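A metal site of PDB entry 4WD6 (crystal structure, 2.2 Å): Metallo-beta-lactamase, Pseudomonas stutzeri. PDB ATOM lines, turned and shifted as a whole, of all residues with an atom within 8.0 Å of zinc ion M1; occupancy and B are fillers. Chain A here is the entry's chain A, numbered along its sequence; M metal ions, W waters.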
ATOM      1  N   TRP A  51      18.706 -23.199 -14.062  1.00  0.00           N
ATOM      2  CA  TRP A  51      18.170 -22.667 -15.318  1.00  0.00           C
ATOM      3  C   TRP A  51      16.711 -22.221 -15.158  1.00  0.00           C
ATOM      4  O   TRP A  51      16.125 -21.839 -16.165  1.00  0.00           O
ATOM      5  CB  TRP A  51      18.296 -23.733 -16.461  1.00  0.00           C
ATOM      6  CG  TRP A  51      18.498 -23.178 -17.851  1.00  0.00           C
ATOM      7  CD1 TRP A  51      18.114 -21.931 -18.317  1.00  0.00           C
ATOM      8  CD2 TRP A  51      19.070 -23.854 -18.999  1.00  0.00           C
ATOM      9  NE1 TRP A  51      18.447 -21.787 -19.636  1.00  0.00           N
ATOM     10  CE2 TRP A  51      19.025 -22.945 -20.092  1.00  0.00           C
ATOM     11  CE3 TRP A  51      19.632 -25.126 -19.204  1.00  0.00           C
ATOM     12  CZ2 TRP A  51      19.530 -23.270 -21.380  1.00  0.00           C
ATOM     13  CZ3 TRP A  51      20.124 -25.457 -20.475  1.00  0.00           C
ATOM     14  CH2 TRP A  51      20.070 -24.530 -21.545  1.00  0.00           C
ATOM     15  N   HIS A  77      29.011 -16.323 -17.190  1.00  0.00           N
ATOM     16  CA  HIS A  77      28.702 -15.523 -18.370  1.00  0.00           C
ATOM     17  C   HIS A  77      27.182 -15.244 -18.343  1.00  0.00           C
ATOM     18  O   HIS A  77      26.470 -15.741 -17.439  1.00  0.00           O
ATOM     19  CB  HIS A  77      29.218 -16.147 -19.700  1.00  0.00           C
ATOM     20  CG  HIS A  77      28.450 -17.333 -20.179  1.00  0.00           C
ATOM     21  ND1 HIS A  77      28.638 -18.585 -19.659  1.00  0.00           N
ATOM     22  CD2 HIS A  77      27.581 -17.469 -21.200  1.00  0.00           C
ATOM     23  CE1 HIS A  77      27.856 -19.441 -20.284  1.00  0.00           C
ATOM     24  NE2 HIS A  77      27.209 -18.781 -21.225  1.00  0.00           N
ATOM     25  N   TRP A  78      26.684 -14.435 -19.258  1.00  0.00           N
ATOM     26  CA  TRP A  78      25.357 -13.837 -19.107  1.00  0.00           C
ATOM     27  C   TRP A  78      24.155 -14.661 -19.490  1.00  0.00           C
ATOM     28  O   TRP A  78      23.007 -14.345 -19.070  1.00  0.00           O
ATOM     29  CB  TRP A  78      25.271 -12.468 -19.815  1.00  0.00           C
ATOM     30  CG  TRP A  78      25.314 -12.487 -21.278  1.00  0.00           C
ATOM     31  CD1 TRP A  78      26.405 -12.492 -22.062  1.00  0.00           C
ATOM     32  CD2 TRP A  78      24.191 -12.435 -22.168  1.00  0.00           C
ATOM     33  NE1 TRP A  78      26.047 -12.472 -23.390  1.00  0.00           N
ATOM     34  CE2 TRP A  78      24.691 -12.427 -23.475  1.00  0.00           C
ATOM     35  CE3 TRP A  78      22.796 -12.385 -21.968  1.00  0.00           C
ATOM     36  CZ2 TRP A  78      23.873 -12.402 -24.596  1.00  0.00           C
ATOM     37  CZ3 TRP A  78      21.986 -12.367 -23.080  1.00  0.00           C
ATOM     38  CH2 TRP A  78      22.517 -12.367 -24.376  1.00  0.00           C
ATOM     39  N   HIS A  79      24.369 -15.679 -20.316  1.00  0.00           N
ATOM     40  CA  HIS A  79      23.235 -16.421 -20.890  1.00  0.00           C
ATOM     41  C   HIS A  79      22.355 -17.041 -19.793  1.00  0.00           C
ATOM     42  O   HIS A  79      22.781 -17.240 -18.636  1.00  0.00           O
ATOM     43  CB  HIS A  79      23.744 -17.512 -21.882  1.00  0.00           C
ATOM     44  CG  HIS A  79      24.382 -16.970 -23.122  1.00  0.00           C
ATOM     45  ND1 HIS A  79      25.354 -17.652 -23.827  1.00  0.00           N
ATOM     46  CD2 HIS A  79      24.240 -15.775 -23.748  1.00  0.00           C
ATOM     47  CE1 HIS A  79      25.750 -16.918 -24.855  1.00  0.00           C
ATOM     48  NE2 HIS A  79      25.093 -15.783 -24.830  1.00  0.00           N
ATOM     49  N   GLU A  80      21.130 -17.376 -20.170  1.00  0.00           N
ATOM     50  CA  GLU A  80      20.126 -17.735 -19.188  1.00  0.00           C
ATOM     51  C   GLU A  80      20.576 -18.910 -18.326  1.00  0.00           C
ATOM     52  O   GLU A  80      20.297 -18.935 -17.143  1.00  0.00           O
ATOM     53  CB  GLU A  80      18.789 -18.085 -19.855  1.00  0.00           C
ATOM     54  CG  GLU A  80      18.073 -16.912 -20.528  1.00  0.00           C
ATOM     55  CD  GLU A  80      16.740 -17.282 -21.151  1.00  0.00           C
ATOM     56  OE1 GLU A  80      16.301 -18.448 -20.957  1.00  0.00           O
ATOM     57  OE2 GLU A  80      16.123 -16.414 -21.834  1.00  0.00           O
ATOM     58  N   ASP A  81      21.264 -19.882 -18.940  1.00  0.00           N
ATOM     59  CA  ASP A  81      21.663 -21.100 -18.203  1.00  0.00           C
ATOM     60  C   ASP A  81      22.569 -20.840 -16.989  1.00  0.00           C
ATOM     61  O   ASP A  81      22.641 -21.652 -16.085  1.00  0.00           O
ATOM     62  CB  ASP A  81      22.250 -22.213 -19.147  1.00  0.00           C
ATOM     63  CG  ASP A  81      23.538 -21.779 -19.871  1.00  0.00           C
ATOM     64  OD1 ASP A  81      23.543 -20.751 -20.558  1.00  0.00           O
ATOM     65  OD2 ASP A  81      24.546 -22.498 -19.772  1.00  0.00           O
ATOM     66  N   ARG A  82      23.240 -19.708 -16.984  1.00  0.00           N
ATOM     67  CA  ARG A  82      24.064 -19.255 -15.878  1.00  0.00           C
ATOM     68  C   ARG A  82      23.389 -18.254 -14.894  1.00  0.00           C
ATOM     69  O   ARG A  82      23.795 -18.147 -13.735  1.00  0.00           O
ATOM     70  CB  ARG A  82      25.284 -18.556 -16.457  1.00  0.00           C
ATOM     71  CG  ARG A  82      26.077 -19.325 -17.512  1.00  0.00           C
ATOM     72  CD  ARG A  82      26.787 -20.511 -16.888  1.00  0.00           C
ATOM     73  NE  ARG A  82      26.274 -21.764 -17.410  1.00  0.00           N
ATOM     74  CZ  ARG A  82      26.420 -22.958 -16.852  1.00  0.00           C
ATOM     75  NH1 ARG A  82      27.047 -23.149 -15.707  1.00  0.00           N
ATOM     76  NH2 ARG A  82      25.897 -24.020 -17.455  1.00  0.00           N
ATOM     77  N   HIS A 139      33.706 -18.898 -25.830  1.00  0.00           N
ATOM     78  CA  HIS A 139      32.258 -19.011 -25.952  1.00  0.00           C
ATOM     79  C   HIS A 139      31.567 -17.652 -26.059  1.00  0.00           C
ATOM     80  O   HIS A 139      30.715 -17.466 -26.900  1.00  0.00           O
ATOM     81  CB  HIS A 139      31.771 -19.728 -24.720  1.00  0.00           C
ATOM     82  CG  HIS A 139      30.293 -19.766 -24.604  1.00  0.00           C
ATOM     83  ND1 HIS A 139      29.513 -20.460 -25.493  1.00  0.00           N
ATOM     84  CD2 HIS A 139      29.448 -19.215 -23.709  1.00  0.00           C
ATOM     85  CE1 HIS A 139      28.246 -20.334 -25.148  1.00  0.00           C
ATOM     86  NE2 HIS A 139      28.178 -19.558 -24.089  1.00  0.00           N
ATOM     87  N   THR A 140      31.949 -16.712 -25.176  1.00  0.00           N
ATOM     88  CA  THR A 140      31.496 -15.319 -25.271  1.00  0.00           C
ATOM     89  C   THR A 140      32.611 -14.445 -24.907  1.00  0.00           C
ATOM     90  O   THR A 140      33.632 -14.919 -24.344  1.00  0.00           O
ATOM     91  CB  THR A 140      30.401 -14.947 -24.264  1.00  0.00           C
ATOM     92  OG1 THR A 140      30.843 -15.268 -22.919  1.00  0.00           O
ATOM     93  CG2 THR A 140      29.133 -15.668 -24.594  1.00  0.00           C
ATOM     94  N   ASP A 142      32.566 -12.357 -22.509  1.00  0.00           N
ATOM     95  CA  ASP A 142      32.588 -12.105 -21.054  1.00  0.00           C
ATOM     96  C   ASP A 142      32.945 -13.339 -20.190  1.00  0.00           C
ATOM     97  O   ASP A 142      33.090 -13.222 -18.976  1.00  0.00           O
ATOM     98  CB  ASP A 142      31.271 -11.501 -20.562  1.00  0.00           C
ATOM     99  CG  ASP A 142      30.070 -12.432 -20.700  1.00  0.00           C
ATOM    100  OD1 ASP A 142      29.289 -12.590 -19.716  1.00  0.00           O
ATOM    101  OD2 ASP A 142      29.871 -12.962 -21.816  1.00  0.00           O
ATOM    102  N   ASN A 143      33.092 -14.504 -20.805  1.00  0.00           N
ATOM    103  CA  ASN A 143      33.194 -15.725 -20.030  1.00  0.00           C
ATOM    104  C   ASN A 143      34.343 -15.755 -19.035  1.00  0.00           C
ATOM    105  O   ASN A 143      35.452 -15.351 -19.351  1.00  0.00           O
ATOM    106  CB  ASN A 143      33.167 -17.006 -20.929  1.00  0.00           C
ATOM    107  CG  ASN A 143      34.258 -17.077 -21.983  1.00  0.00           C
ATOM    108  OD1 ASN A 143      34.151 -17.882 -22.884  1.00  0.00           O
ATOM    109  ND2 ASN A 143      35.331 -16.329 -21.853  1.00  0.00           N
ATOM    110  N   CYS A 158      30.866 -22.695 -19.544  1.00  0.00           N
ATOM    111  CA  CYS A 158      30.666 -23.031 -20.951  1.00  0.00           C
ATOM    112  C   CYS A 158      31.842 -22.612 -21.835  1.00  0.00           C
ATOM    113  O   CYS A 158      31.865 -22.920 -23.007  1.00  0.00           O
ATOM    114  CB  CYS A 158      29.369 -22.411 -21.421  1.00  0.00           C
ATOM    115  SG  CYS A 158      27.964 -22.827 -20.341  1.00  0.00           S
ATOM    116  N   PHE A 159      32.851 -21.986 -21.228  1.00  0.00           N
ATOM    117  CA  PHE A 159      34.193 -21.833 -21.830  1.00  0.00           C
ATOM    118  C   PHE A 159      34.956 -23.163 -22.134  1.00  0.00           C
ATOM    119  O   PHE A 159      35.858 -23.193 -22.972  1.00  0.00           O
ATOM    120  CB  PHE A 159      35.010 -20.907 -20.906  1.00  0.00           C
ATOM    121  CG  PHE A 159      36.402 -20.679 -21.377  1.00  0.00           C
ATOM    122  CD1 PHE A 159      37.458 -21.365 -20.803  1.00  0.00           C
ATOM    123  CD2 PHE A 159      36.674 -19.714 -22.339  1.00  0.00           C
ATOM    124  CE1 PHE A 159      38.762 -21.151 -21.249  1.00  0.00           C
ATOM    125  CE2 PHE A 159      37.969 -19.504 -22.781  1.00  0.00           C
ATOM    126  CZ  PHE A 159      39.014 -20.228 -22.241  1.00  0.00           C
ATOM    127  N   TYR A 170      26.837 -23.452 -29.358  1.00  0.00           N
ATOM    128  CA  TYR A 170      26.390 -22.200 -29.985  1.00  0.00           C
ATOM    129  C   TYR A 170      27.585 -21.219 -30.101  1.00  0.00           C
ATOM    130  O   TYR A 170      28.184 -20.837 -29.092  1.00  0.00           O
ATOM    131  CB  TYR A 170      25.183 -21.583 -29.212  1.00  0.00           C
ATOM    132  CG  TYR A 170      24.922 -20.144 -29.539  1.00  0.00           C
ATOM    133  CD1 TYR A 170      24.185 -19.771 -30.682  1.00  0.00           C
ATOM    134  CD2 TYR A 170      25.417 -19.124 -28.724  1.00  0.00           C
ATOM    135  CE1 TYR A 170      23.954 -18.439 -30.992  1.00  0.00           C
ATOM    136  CE2 TYR A 170      25.198 -17.788 -29.028  1.00  0.00           C
ATOM    137  CZ  TYR A 170      24.455 -17.438 -30.154  1.00  0.00           C
ATOM    138  OH  TYR A 170      24.267 -16.110 -30.448  1.00  0.00           O
ATOM    139  N   GLU A 173      28.007 -15.948 -30.733  1.00  0.00           N
ATOM    140  CA  GLU A 173      28.635 -14.809 -30.085  1.00  0.00           C
ATOM    141  C   GLU A 173      30.065 -15.104 -29.728  1.00  0.00           C
ATOM    142  O   GLU A 173      30.692 -14.333 -28.977  1.00  0.00           O
ATOM    143  CB  GLU A 173      27.868 -14.419 -28.827  1.00  0.00           C
ATOM    144  CG  GLU A 173      26.473 -13.840 -29.080  1.00  0.00           C
ATOM    145  CD  GLU A 173      25.569 -14.113 -27.901  1.00  0.00           C
ATOM    146  OE1 GLU A 173      25.887 -13.685 -26.771  1.00  0.00           O
ATOM    147  OE2 GLU A 173      24.561 -14.812 -28.075  1.00  0.00           O
ATOM    148  N   HIS A 200      28.212 -27.917 -19.431  1.00  0.00           N
ATOM    149  CA  HIS A 200      27.292 -28.960 -19.908  1.00  0.00           C
ATOM    150  C   HIS A 200      28.101 -30.238 -20.011  1.00  0.00           C
ATOM    151  O   HIS A 200      29.193 -30.242 -20.557  1.00  0.00           O
ATOM    152  CB  HIS A 200      26.771 -28.584 -21.274  1.00  0.00           C
ATOM    153  CG  HIS A 200      26.136 -27.246 -21.302  1.00  0.00           C
ATOM    154  ND1 HIS A 200      24.844 -27.032 -20.853  1.00  0.00           N
ATOM    155  CD2 HIS A 200      26.626 -26.026 -21.620  1.00  0.00           C
ATOM    156  CE1 HIS A 200      24.570 -25.739 -20.925  1.00  0.00           C
ATOM    157  NE2 HIS A 200      25.620 -25.122 -21.436  1.00  0.00           N
HETATM  158 ZN    ZN M   1      26.237 -19.417 -23.274  1.00  0.00          ZN
HETATM  159 ZN    ZN M   2      26.097 -22.933 -21.441  1.00  0.00          ZN
HETATM  160  O   HOH W   1      24.919 -20.650 -25.050  1.00  0.00           O
HETATM  161  O   HOH W   2      25.475 -20.987 -22.762  1.00  0.00           O
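Zinc ion M1 is bound by water W2 (1.8 Å), a ring nitrogen (ND1) of His 79 (2.0 Å), a ring nitrogen (NE2) of His 139 (2.1 Å), a ring nitrogen (NE2) of His 77 (2.4 Å) and water W1 (2.5 Å).
Of the 16 residues printed, 3 come within 4 Å of zinc ion M1. Along chain A the residues within 4 Å of zinc ion M1 span positions 77 to 139. The nearest printed residue that does not touch zinc ion M1 is Asp 81 (4.1 Å).
A ring nitrogen (NE2) of His 79 sits at hydrogen-bond distance from the side-chain carboxylate of Glu 173, 3.0 Å away. The side-chain amide oxygen (OD1) of Asn 143 sits at hydrogen-bond distance from the backbone NH (N) of His 139, at 3.1 Å.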
